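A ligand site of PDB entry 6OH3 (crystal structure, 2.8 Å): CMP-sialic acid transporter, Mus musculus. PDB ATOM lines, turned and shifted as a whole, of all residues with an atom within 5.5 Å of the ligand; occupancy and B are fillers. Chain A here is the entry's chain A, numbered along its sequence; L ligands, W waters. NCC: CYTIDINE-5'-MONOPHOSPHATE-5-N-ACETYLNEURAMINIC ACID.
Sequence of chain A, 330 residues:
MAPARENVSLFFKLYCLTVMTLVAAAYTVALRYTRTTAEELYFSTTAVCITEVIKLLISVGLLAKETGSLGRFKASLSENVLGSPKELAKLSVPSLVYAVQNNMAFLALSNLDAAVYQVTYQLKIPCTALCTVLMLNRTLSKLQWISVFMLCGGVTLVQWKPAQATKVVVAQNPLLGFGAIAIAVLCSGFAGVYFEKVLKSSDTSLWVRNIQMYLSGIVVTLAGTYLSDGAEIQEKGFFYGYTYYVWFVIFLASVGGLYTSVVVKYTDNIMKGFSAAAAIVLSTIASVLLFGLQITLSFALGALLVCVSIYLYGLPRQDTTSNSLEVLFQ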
ATOM      1  N   MET A  20      13.743 -17.862  -3.213  1.00  0.00           N
ATOM      2  CA  MET A  20      13.172 -16.648  -2.602  1.00  0.00           C
ATOM      3  C   MET A  20      11.843 -16.917  -1.889  1.00  0.00           C
ATOM      4  O   MET A  20      11.633 -16.428  -0.769  1.00  0.00           O
ATOM      5  CB  MET A  20      12.983 -15.552  -3.658  1.00  0.00           C
ATOM      6  CG  MET A  20      12.228 -14.311  -3.184  1.00  0.00           C
ATOM      7  SD  MET A  20      11.871 -13.150  -4.513  1.00  0.00           S
ATOM      8  CE  MET A  20      10.273 -12.507  -4.031  1.00  0.00           C
ATOM      9  N   VAL A  23      12.330 -19.632   1.073  1.00  0.00           N
ATOM     10  CA  VAL A  23      12.956 -18.899   2.180  1.00  0.00           C
ATOM     11  C   VAL A  23      11.965 -17.933   2.830  1.00  0.00           C
ATOM     12  O   VAL A  23      11.900 -17.855   4.058  1.00  0.00           O
ATOM     13  CB  VAL A  23      14.234 -18.140   1.725  1.00  0.00           C
ATOM     14  CG1 VAL A  23      14.711 -17.136   2.764  1.00  0.00           C
ATOM     15  CG2 VAL A  23      15.347 -19.136   1.413  1.00  0.00           C
ATOM     16  N   ALA A  24      11.193 -17.204   2.015  1.00  0.00           N
ATOM     17  CA  ALA A  24      10.158 -16.301   2.536  1.00  0.00           C
ATOM     18  C   ALA A  24       9.111 -17.026   3.390  1.00  0.00           C
ATOM     19  O   ALA A  24       8.705 -16.525   4.432  1.00  0.00           O
ATOM     20  CB  ALA A  24       9.485 -15.552   1.394  1.00  0.00           C
ATOM     21  N   TYR A  27      10.958 -18.208   6.553  1.00  0.00           N
ATOM     22  CA  TYR A  27      11.388 -17.037   7.342  1.00  0.00           C
ATOM     23  C   TYR A  27      10.319 -16.573   8.333  1.00  0.00           C
ATOM     24  O   TYR A  27      10.620 -16.367   9.515  1.00  0.00           O
ATOM     25  CB  TYR A  27      11.775 -15.885   6.403  1.00  0.00           C
ATOM     26  CG  TYR A  27      12.080 -14.566   7.076  1.00  0.00           C
ATOM     27  CD1 TYR A  27      13.242 -14.388   7.830  1.00  0.00           C
ATOM     28  CD2 TYR A  27      11.209 -13.476   6.938  1.00  0.00           C
ATOM     29  CE1 TYR A  27      13.518 -13.178   8.442  1.00  0.00           C
ATOM     30  CE2 TYR A  27      11.471 -12.262   7.547  1.00  0.00           C
ATOM     31  CZ  TYR A  27      12.629 -12.110   8.290  1.00  0.00           C
ATOM     32  OH  TYR A  27      12.893 -10.906   8.884  1.00  0.00           O
ATOM     33  N   THR A  28       9.087 -16.419   7.853  1.00  0.00           N
ATOM     34  CA  THR A  28       7.969 -15.971   8.697  1.00  0.00           C
ATOM     35  C   THR A  28       7.574 -16.965   9.780  1.00  0.00           C
ATOM     36  O   THR A  28       7.155 -16.575  10.868  1.00  0.00           O
ATOM     37  CB  THR A  28       6.722 -15.651   7.844  1.00  0.00           C
ATOM     38  OG1 THR A  28       6.363 -16.800   7.066  1.00  0.00           O
ATOM     39  CG2 THR A  28       6.984 -14.474   6.913  1.00  0.00           C
ATOM     40  N   GLU A  52      22.293  -7.236   7.781  1.00  0.00           N
ATOM     41  CA  GLU A  52      22.952  -6.259   6.888  1.00  0.00           C
ATOM     42  C   GLU A  52      24.462  -6.462   6.801  1.00  0.00           C
ATOM     43  O   GLU A  52      25.063  -6.182   5.761  1.00  0.00           O
ATOM     44  CB  GLU A  52      22.672  -4.821   7.347  1.00  0.00           C
ATOM     45  CG  GLU A  52      21.203  -4.398   7.337  1.00  0.00           C
ATOM     46  CD  GLU A  52      20.609  -4.388   5.947  1.00  0.00           C
ATOM     47  OE1 GLU A  52      21.163  -3.698   5.059  1.00  0.00           O
ATOM     48  OE2 GLU A  52      19.572  -5.067   5.743  1.00  0.00           O
ATOM     49  N   LYS A  55      24.672  -9.851   4.674  1.00  0.00           N
ATOM     50  CA  LYS A  55      24.347  -9.529   3.280  1.00  0.00           C
ATOM     51  C   LYS A  55      25.470  -8.771   2.578  1.00  0.00           C
ATOM     52  O   LYS A  55      25.777  -9.034   1.416  1.00  0.00           O
ATOM     53  CB  LYS A  55      23.056  -8.711   3.184  1.00  0.00           C
ATOM     54  CG  LYS A  55      21.788  -9.509   3.415  1.00  0.00           C
ATOM     55  CD  LYS A  55      20.553  -8.745   2.961  1.00  0.00           C
ATOM     56  CE  LYS A  55      20.353  -7.450   3.746  1.00  0.00           C
ATOM     57  NZ  LYS A  55      19.007  -6.849   3.542  1.00  0.00           N
ATOM     58  N   TYR A  98      14.063   0.290   4.243  1.00  0.00           N
ATOM     59  CA  TYR A  98      14.179  -1.142   4.557  1.00  0.00           C
ATOM     60  C   TYR A  98      14.533  -1.403   6.017  1.00  0.00           C
ATOM     61  O   TYR A  98      14.084  -2.397   6.587  1.00  0.00           O
ATOM     62  CB  TYR A  98      15.228  -1.849   3.674  1.00  0.00           C
ATOM     63  CG  TYR A  98      14.758  -2.213   2.273  1.00  0.00           C
ATOM     64  CD1 TYR A  98      13.522  -2.819   2.068  1.00  0.00           C
ATOM     65  CD2 TYR A  98      15.571  -2.001   1.162  1.00  0.00           C
ATOM     66  CE1 TYR A  98      13.085  -3.166   0.798  1.00  0.00           C
ATOM     67  CE2 TYR A  98      15.142  -2.353  -0.119  1.00  0.00           C
ATOM     68  CZ  TYR A  98      13.898  -2.931  -0.294  1.00  0.00           C
ATOM     69  OH  TYR A  98      13.489  -3.272  -1.552  1.00  0.00           O
ATOM     70  N   GLN A 101      11.273  -1.174   7.579  1.00  0.00           N
ATOM     71  CA  GLN A 101      10.513  -2.350   7.118  1.00  0.00           C
ATOM     72  C   GLN A 101      10.893  -3.621   7.866  1.00  0.00           C
ATOM     73  O   GLN A 101      10.027  -4.288   8.435  1.00  0.00           O
ATOM     74  CB  GLN A 101      10.737  -2.603   5.615  1.00  0.00           C
ATOM     75  CG  GLN A 101       9.994  -3.829   5.064  1.00  0.00           C
ATOM     76  CD  GLN A 101      10.076  -3.972   3.560  1.00  0.00           C
ATOM     77  OE1 GLN A 101      10.434  -3.035   2.847  1.00  0.00           O
ATOM     78  NE2 GLN A 101       9.725  -5.149   3.067  1.00  0.00           N
ATOM     79  N   ASN A 102      12.187  -3.918   7.869  1.00  0.00           N
ATOM     80  CA  ASN A 102      12.704  -5.144   8.492  1.00  0.00           C
ATOM     81  C   ASN A 102      12.453  -5.174   9.995  1.00  0.00           C
ATOM     82  O   ASN A 102      12.206  -6.238  10.557  1.00  0.00           O
ATOM     83  CB  ASN A 102      14.193  -5.325   8.192  1.00  0.00           C
ATOM     84  CG  ASN A 102      14.467  -5.523   6.705  1.00  0.00           C
ATOM     85  OD1 ASN A 102      13.814  -6.328   6.056  1.00  0.00           O
ATOM     86  ND2 ASN A 102      15.434  -4.781   6.176  1.00  0.00           N
ATOM     87  N   ALA A 105       8.756  -5.867  10.361  1.00  0.00           N
ATOM     88  CA  ALA A 105       8.534  -7.301  10.114  1.00  0.00           C
ATOM     89  C   ALA A 105       8.695  -8.129  11.391  1.00  0.00           C
ATOM     90  O   ALA A 105       7.892  -9.020  11.656  1.00  0.00           O
ATOM     91  CB  ALA A 105       9.483  -7.811   9.040  1.00  0.00           C
ATOM     92  N   LEU A 109       5.264 -10.029  13.473  1.00  0.00           N
ATOM     93  CA  LEU A 109       5.257 -11.470  13.784  1.00  0.00           C
ATOM     94  C   LEU A 109       5.420 -11.791  15.277  1.00  0.00           C
ATOM     95  O   LEU A 109       5.074 -12.893  15.711  1.00  0.00           O
ATOM     96  CB  LEU A 109       6.336 -12.190  12.974  1.00  0.00           C
ATOM     97  CG  LEU A 109       6.090 -12.188  11.461  1.00  0.00           C
ATOM     98  CD1 LEU A 109       7.388 -12.429  10.699  1.00  0.00           C
ATOM     99  CD2 LEU A 109       5.040 -13.227  11.067  1.00  0.00           C
ATOM    100  N   TYR A 117      -0.145 -12.683   9.328  1.00  0.00           N
ATOM    101  CA  TYR A 117       0.846 -11.752   8.763  1.00  0.00           C
ATOM    102  C   TYR A 117       0.952 -11.876   7.242  1.00  0.00           C
ATOM    103  O   TYR A 117       0.902 -10.874   6.539  1.00  0.00           O
ATOM    104  CB  TYR A 117       2.226 -11.959   9.402  1.00  0.00           C
ATOM    105  CG  TYR A 117       3.352 -11.190   8.727  1.00  0.00           C
ATOM    106  CD1 TYR A 117       3.617  -9.860   9.076  1.00  0.00           C
ATOM    107  CD2 TYR A 117       4.154 -11.785   7.750  1.00  0.00           C
ATOM    108  CE1 TYR A 117       4.651  -9.148   8.460  1.00  0.00           C
ATOM    109  CE2 TYR A 117       5.180 -11.077   7.129  1.00  0.00           C
ATOM    110  CZ  TYR A 117       5.423  -9.763   7.487  1.00  0.00           C
ATOM    111  OH  TYR A 117       6.444  -9.071   6.870  1.00  0.00           O
ATOM    112  N   TYR A 121       0.019  -8.924   4.561  1.00  0.00           N
ATOM    113  CA  TYR A 121       1.189  -8.344   3.891  1.00  0.00           C
ATOM    114  C   TYR A 121       1.120  -8.390   2.346  1.00  0.00           C
ATOM    115  O   TYR A 121       1.902  -7.695   1.689  1.00  0.00           O
ATOM    116  CB  TYR A 121       2.464  -9.038   4.385  1.00  0.00           C
ATOM    117  CG  TYR A 121       3.769  -8.346   4.040  1.00  0.00           C
ATOM    118  CD1 TYR A 121       3.985  -7.014   4.405  1.00  0.00           C
ATOM    119  CD2 TYR A 121       4.783  -9.015   3.359  1.00  0.00           C
ATOM    120  CE1 TYR A 121       5.177  -6.377   4.088  1.00  0.00           C
ATOM    121  CE2 TYR A 121       5.975  -8.378   3.043  1.00  0.00           C
ATOM    122  CZ  TYR A 121       6.169  -7.062   3.416  1.00  0.00           C
ATOM    123  OH  TYR A 121       7.350  -6.432   3.105  1.00  0.00           O
ATOM    124  N   LYS A 124       0.959  -5.226  -0.114  1.00  0.00           N
ATOM    125  CA  LYS A 124       2.147  -4.681  -0.801  1.00  0.00           C
ATOM    126  C   LYS A 124       2.039  -4.742  -2.332  1.00  0.00           C
ATOM    127  O   LYS A 124       2.646  -3.919  -3.019  1.00  0.00           O
ATOM    128  CB  LYS A 124       3.428  -5.425  -0.357  1.00  0.00           C
ATOM    129  CG  LYS A 124       3.558  -6.825  -0.958  1.00  0.00           C
ATOM    130  CD  LYS A 124       4.485  -7.747  -0.189  1.00  0.00           C
ATOM    131  CE  LYS A 124       4.096  -9.205  -0.460  1.00  0.00           C
ATOM    132  NZ  LYS A 124       4.954 -10.210   0.220  1.00  0.00           N
ATOM    133  N   SER A 188       7.930  -1.545   1.565  1.00  0.00           N
ATOM    134  CA  SER A 188       8.248  -2.567   0.562  1.00  0.00           C
ATOM    135  C   SER A 188       8.058  -2.068  -0.865  1.00  0.00           C
ATOM    136  O   SER A 188       8.937  -2.253  -1.702  1.00  0.00           O
ATOM    137  CB  SER A 188       7.379  -3.812   0.789  1.00  0.00           C
ATOM    138  OG  SER A 188       7.726  -4.851  -0.109  1.00  0.00           O
ATOM    139  N   PHE A 195      15.004   0.993  -5.445  1.00  0.00           N
ATOM    140  CA  PHE A 195      16.164   0.161  -5.761  1.00  0.00           C
ATOM    141  C   PHE A 195      16.169  -0.303  -7.227  1.00  0.00           C
ATOM    142  O   PHE A 195      17.228  -0.322  -7.850  1.00  0.00           O
ATOM    143  CB  PHE A 195      16.287  -1.060  -4.841  1.00  0.00           C
ATOM    144  CG  PHE A 195      17.549  -1.869  -5.089  1.00  0.00           C
ATOM    145  CD1 PHE A 195      18.753  -1.472  -4.522  1.00  0.00           C
ATOM    146  CD2 PHE A 195      17.528  -2.993  -5.915  1.00  0.00           C
ATOM    147  CE1 PHE A 195      19.920  -2.201  -4.754  1.00  0.00           C
ATOM    148  CE2 PHE A 195      18.674  -3.723  -6.155  1.00  0.00           C
ATOM    149  CZ  PHE A 195      19.882  -3.325  -5.574  1.00  0.00           C
ATOM    150  N   ASN A 210      24.050  -3.504  -4.275  1.00  0.00           N
ATOM    151  CA  ASN A 210      23.809  -4.130  -2.982  1.00  0.00           C
ATOM    152  C   ASN A 210      24.782  -3.645  -1.905  1.00  0.00           C
ATOM    153  O   ASN A 210      24.359  -3.295  -0.811  1.00  0.00           O
ATOM    154  CB  ASN A 210      23.874  -5.666  -3.105  1.00  0.00           C
ATOM    155  CG  ASN A 210      22.623  -6.266  -3.739  1.00  0.00           C
ATOM    156  OD1 ASN A 210      21.616  -5.585  -3.939  1.00  0.00           O
ATOM    157  ND2 ASN A 210      22.685  -7.554  -4.044  1.00  0.00           N
ATOM    158  N   MET A 213      24.090  -0.076  -0.865  1.00  0.00           N
ATOM    159  CA  MET A 213      22.894  -0.028  -0.035  1.00  0.00           C
ATOM    160  C   MET A 213      23.157  -0.540   1.392  1.00  0.00           C
ATOM    161  O   MET A 213      22.747   0.112   2.353  1.00  0.00           O
ATOM    162  CB  MET A 213      21.783  -0.862  -0.669  1.00  0.00           C
ATOM    163  CG  MET A 213      20.396  -0.545  -0.126  1.00  0.00           C
ATOM    164  SD  MET A 213      19.205  -1.800  -0.615  1.00  0.00           S
ATOM    165  CE  MET A 213      17.918  -0.765  -1.305  1.00  0.00           C
ATOM    166  N   TYR A 214      23.805  -1.691   1.506  1.00  0.00           N
ATOM    167  CA  TYR A 214      24.016  -2.333   2.822  1.00  0.00           C
ATOM    168  C   TYR A 214      25.032  -1.590   3.693  1.00  0.00           C
ATOM    169  O   TYR A 214      24.961  -1.673   4.917  1.00  0.00           O
ATOM    170  CB  TYR A 214      24.435  -3.811   2.680  1.00  0.00           C
ATOM    171  CG  TYR A 214      23.540  -4.680   1.819  1.00  0.00           C
ATOM    172  CD1 TYR A 214      22.159  -4.454   1.726  1.00  0.00           C
ATOM    173  CD2 TYR A 214      24.074  -5.735   1.085  1.00  0.00           C
ATOM    174  CE1 TYR A 214      21.347  -5.263   0.928  1.00  0.00           C
ATOM    175  CE2 TYR A 214      23.270  -6.539   0.292  1.00  0.00           C
ATOM    176  CZ  TYR A 214      21.912  -6.299   0.211  1.00  0.00           C
ATOM    177  OH  TYR A 214      21.137  -7.107  -0.583  1.00  0.00           O
ATOM    178  N   LEU A 252      18.419 -16.929   7.009  1.00  0.00           N
ATOM    179  CA  LEU A 252      17.345 -16.862   6.005  1.00  0.00           C
ATOM    180  C   LEU A 252      17.057 -15.430   5.539  1.00  0.00           C
ATOM    181  O   LEU A 252      16.751 -15.207   4.374  1.00  0.00           O
ATOM    182  CB  LEU A 252      16.050 -17.473   6.540  1.00  0.00           C
ATOM    183  CG  LEU A 252      15.994 -18.985   6.763  1.00  0.00           C
ATOM    184  CD1 LEU A 252      14.683 -19.346   7.449  1.00  0.00           C
ATOM    185  CD2 LEU A 252      16.139 -19.748   5.453  1.00  0.00           C
ATOM    186  N   ALA A 253      17.144 -14.467   6.465  1.00  0.00           N
ATOM    187  CA  ALA A 253      16.972 -13.048   6.149  1.00  0.00           C
ATOM    188  C   ALA A 253      18.070 -12.545   5.211  1.00  0.00           C
ATOM    189  O   ALA A 253      17.811 -11.732   4.321  1.00  0.00           O
ATOM    190  CB  ALA A 253      16.941 -12.215   7.413  1.00  0.00           C
ATOM    191  N   GLY A 256      17.500 -14.557   1.747  1.00  0.00           N
ATOM    192  CA  GLY A 256      16.255 -14.061   1.160  1.00  0.00           C
ATOM    193  C   GLY A 256      16.324 -12.665   0.563  1.00  0.00           C
ATOM    194  O   GLY A 256      15.683 -12.383  -0.444  1.00  0.00           O
ATOM    195  N   GLY A 257      17.109 -11.784   1.196  1.00  0.00           N
ATOM    196  CA  GLY A 257      17.325 -10.432   0.682  1.00  0.00           C
ATOM    197  C   GLY A 257      18.161 -10.391  -0.583  1.00  0.00           C
ATOM    198  O   GLY A 257      17.842  -9.649  -1.521  1.00  0.00           O
ATOM    199  N   LEU A 258      19.237 -11.169  -0.607  1.00  0.00           N
ATOM    200  CA  LEU A 258      20.111 -11.258  -1.782  1.00  0.00           C
ATOM    201  C   LEU A 258      19.385 -11.827  -3.000  1.00  0.00           C
ATOM    202  O   LEU A 258      19.584 -11.346  -4.114  1.00  0.00           O
ATOM    203  CB  LEU A 258      21.348 -12.100  -1.478  1.00  0.00           C
ATOM    204  CG  LEU A 258      22.323 -11.510  -0.465  1.00  0.00           C
ATOM    205  CD1 LEU A 258      23.279 -12.574   0.039  1.00  0.00           C
ATOM    206  CD2 LEU A 258      23.102 -10.342  -1.065  1.00  0.00           C
ATOM    207  N   THR A 260      16.066 -11.653  -3.557  1.00  0.00           N
ATOM    208  CA  THR A 260      15.088 -10.645  -4.010  1.00  0.00           C
ATOM    209  C   THR A 260      15.722  -9.599  -4.909  1.00  0.00           C
ATOM    210  O   THR A 260      15.095  -9.143  -5.871  1.00  0.00           O
ATOM    211  CB  THR A 260      14.372  -9.944  -2.839  1.00  0.00           C
ATOM    212  OG1 THR A 260      15.327  -9.391  -1.936  1.00  0.00           O
ATOM    213  CG2 THR A 260      13.474 -10.918  -2.099  1.00  0.00           C
ATOM    214  N   SER A 261      16.971  -9.214  -4.610  1.00  0.00           N
ATOM    215  CA  SER A 261      17.718  -8.289  -5.467  1.00  0.00           C
ATOM    216  C   SER A 261      17.967  -8.877  -6.867  1.00  0.00           C
ATOM    217  O   SER A 261      17.851  -8.173  -7.869  1.00  0.00           O
ATOM    218  CB  SER A 261      19.048  -7.879  -4.816  1.00  0.00           C
ATOM    219  OG  SER A 261      19.993  -8.937  -4.842  1.00  0.00           O
ATOM    220  N   LYS A 272       7.562  -9.694  -9.639  1.00  0.00           N
ATOM    221  CA  LYS A 272       8.002 -10.400  -8.431  1.00  0.00           C
ATOM    222  C   LYS A 272       6.811 -10.982  -7.656  1.00  0.00           C
ATOM    223  O   LYS A 272       6.878 -12.105  -7.171  1.00  0.00           O
ATOM    224  CB  LYS A 272       8.813  -9.461  -7.519  1.00  0.00           C
ATOM    225  CG  LYS A 272       9.524 -10.138  -6.360  1.00  0.00           C
ATOM    226  CD  LYS A 272      10.263  -9.106  -5.509  1.00  0.00           C
ATOM    227  CE  LYS A 272       9.340  -8.451  -4.497  1.00  0.00           C
ATOM    228  NZ  LYS A 272       9.813  -7.096  -4.109  1.00  0.00           N
HETATM  229  O3P NCC L   1       9.171  -7.221   1.125  1.00  0.00           O
HETATM  230  P   NCC L   1      10.050  -7.375  -0.082  1.00  0.00           P
HETATM  231  O2P NCC L   1      10.094  -8.902  -0.603  1.00  0.00           O
HETATM  232  O1P NCC L   1       9.808  -6.490  -1.278  1.00  0.00           O
HETATM  233  O5' NCC L   1      11.615  -7.222   0.292  1.00  0.00           O
HETATM  234  C5' NCC L   1      12.111  -6.801   1.566  1.00  0.00           C
HETATM  235  C4' NCC L   1      13.442  -7.485   1.881  1.00  0.00           C
HETATM  236  O4' NCC L   1      14.283  -7.573   0.718  1.00  0.00           O
HETATM  237  C1' NCC L   1      15.590  -7.122   1.095  1.00  0.00           C
HETATM  238  N1  NCC L   1      16.385  -6.560  -0.010  1.00  0.00           N
HETATM  239  C6  NCC L   1      15.801  -5.912  -1.022  1.00  0.00           C
HETATM  240  C5  NCC L   1      16.573  -5.397  -2.061  1.00  0.00           C
HETATM  241  C4  NCC L   1      17.957  -5.555  -2.020  1.00  0.00           C
HETATM  242  N4  NCC L   1      18.721  -5.051  -3.011  1.00  0.00           N
HETATM  243  N3  NCC L   1      18.545  -6.201  -0.995  1.00  0.00           N
HETATM  244  C2  NCC L   1      17.802  -6.704   0.003  1.00  0.00           C
HETATM  245  O2  NCC L   1      18.391  -7.303   0.933  1.00  0.00           O
HETATM  246  C2' NCC L   1      15.338  -6.062   2.147  1.00  0.00           C
HETATM  247  O2' NCC L   1      16.493  -5.785   2.945  1.00  0.00           O
HETATM  248  C3' NCC L   1      14.216  -6.707   2.934  1.00  0.00           C
HETATM  249  O3' NCC L   1      14.728  -7.594   3.935  1.00  0.00           O
HETATM  250  C9  NCC L   1       8.025 -10.048  -0.922  1.00  0.00           C
HETATM  251  O1B NCC L   1       7.700  -9.070  -1.643  1.00  0.00           O
HETATM  252  O1A NCC L   1       7.271 -11.046  -0.812  1.00  0.00           O
HETATM  253  C10 NCC L   1       9.320 -10.015  -0.138  1.00  0.00           C
HETATM  254  O6  NCC L   1       9.008  -9.953   1.264  1.00  0.00           O
HETATM  255  C12 NCC L   1      10.073 -10.082   2.233  1.00  0.00           C
HETATM  256  C13 NCC L   1       9.342  -9.883   3.588  1.00  0.00           C
HETATM  257  O7  NCC L   1       9.042  -8.488   3.677  1.00  0.00           O
HETATM  258  C14 NCC L   1      10.021 -10.285   4.902  1.00  0.00           C
HETATM  259  O8  NCC L   1       8.975 -10.503   5.859  1.00  0.00           O
HETATM  260  C15 NCC L   1      10.970  -9.240   5.486  1.00  0.00           C
HETATM  261  O9  NCC L   1      11.789  -8.625   4.488  1.00  0.00           O
HETATM  262  C16 NCC L   1      10.872 -11.370   2.004  1.00  0.00           C
HETATM  263  N5  NCC L   1      12.083 -11.420   2.817  1.00  0.00           N
HETATM  264  C17 NCC L   1      12.715 -12.546   3.137  1.00  0.00           C
HETATM  265  O10 NCC L   1      12.350 -13.654   2.798  1.00  0.00           O
HETATM  266  C18 NCC L   1      13.964 -12.378   3.952  1.00  0.00           C
HETATM  267  C19 NCC L   1      11.301 -11.431   0.533  1.00  0.00           C
HETATM  268  O4  NCC L   1      11.994 -12.658   0.220  1.00  0.00           O
HETATM  269  C20 NCC L   1      10.116 -11.300  -0.411  1.00  0.00           C
HETATM  270  O   HOH W   1      10.902  -4.098  -1.371  1.00  0.00           O
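The side-chain amide oxygen (OD1) of Asn 102 lies within hydrogen-bond range of an oxygen (O3') of the ligand (2.6 Å).
The side-chain amino group (NZ) of Lys 124 is in salt-bridge range of an oxygen (O1A) of the ligand (2.7 Å).
NZ of Lys 55 lies within hydrogen-bond range of O2 of the ligand, at 2.7 Å.
An oxygen (O7) of the ligand is in hydrogen-bond range of the side-chain hydroxyl (OH) of Tyr 121 (2.7 Å).
The side-chain hydroxyl (OH) of Tyr 214 lies within hydrogen-bond range of a nitrogen (N3) of the ligand, 2.8 Å away.
An oxygen (O3P) of the ligand lies within hydrogen-bond range of the side-chain amide nitrogen (NE2) of Gln 101, at 2.9 Å.
The side-chain amino group (NZ) of Lys 272 is in salt-bridge range of an oxygen (O1P) of the ligand, 2.9 Å away.
O1P of the ligand lies within hydrogen-bond range of OG of Ser 188, at 2.9 Å.
The side-chain hydroxyl (OH) of Tyr 117 lies within hydrogen-bond range of an oxygen (O8) of the ligand (3.1 Å).
The side-chain amide oxygen (OD1) of Asn 210 sits at hydrogen-bond distance from a nitrogen (N4) of the ligand (3.1 Å).
The side-chain hydroxyl (OG1) of Thr 260 is in hydrogen-bond range of an oxygen (O4') of the ligand (3.4 Å).
ND2 of Asn 102 sits at hydrogen-bond distance from O of Tyr 98 (2.8 Å).
The side-chain amino group of Lys 55 lies within salt-bridge range of the side-chain carboxylate of Glu 52, at 2.9 Å.
The side-chain amide nitrogen of Gln 101 lies within hydrogen-bond range of the side-chain hydroxyl of Tyr 121 (2.7 Å).
N of Ser 188 lies within hydrogen-bond range of OE1 of Gln 101 (3.2 Å).
OG of Ser 261 lies within hydrogen-bond range of ND2 of Asn 210 (3.1 Å).
The backbone carbonyl oxygen of Gly 257 is in hydrogen-bond range of the side-chain hydroxyl of Thr 260, at 2.6 Å.
The side-chain hydroxyl (OG1) of Thr 260 lies close to the backbone carbonyl oxygen (O) of Gly 256 (3.4 Å).
The backbone carbonyl oxygen (O) of Leu 258 lies within hydrogen-bond range of the side-chain hydroxyl (OG) of Ser 261 (2.5 Å).
O of Gly 257 sits close to O2 of the ligand (3.4 Å).
Merely in contact with the ligand: Phe 195 (3.3 Å), Ser 261 (3.4 Å), Ala 24 (3.4 Å), Tyr 27 (3.5 Å), Tyr 98 (3.5 Å), Gly 256 (3.8 Å), Ala 253 (3.8 Å), Met 20 (3.8 Å) and Leu 252 (3.99 Å).
Hydrophobic or aromatic side chains within 4 Å of the ligand: Met 20, Ala 24, Tyr 27, Tyr 98, Tyr 117, Tyr 121, Phe 195 and Tyr 214.
Within 4 Å of the ligand: Met 20, Ala 24, Tyr 27, Lys 55, Tyr 98, Gln 101, Asn 102, Tyr 117, Tyr 121, Lys 124, Ser 188, Phe 195, Asn 210, Tyr 214, Leu 252, Ala 253, Gly 256, Gly 257, Thr 260, Ser 261 and Lys 272.
Water W1 lies within hydrogen-bond range of an oxygen (O1P) of the ligand (2.6 Å), the backbone carbonyl oxygen (O) of Ser 188 (2.7 Å) and the side-chain hydroxyl (OH) of Tyr 98 (2.7 Å).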
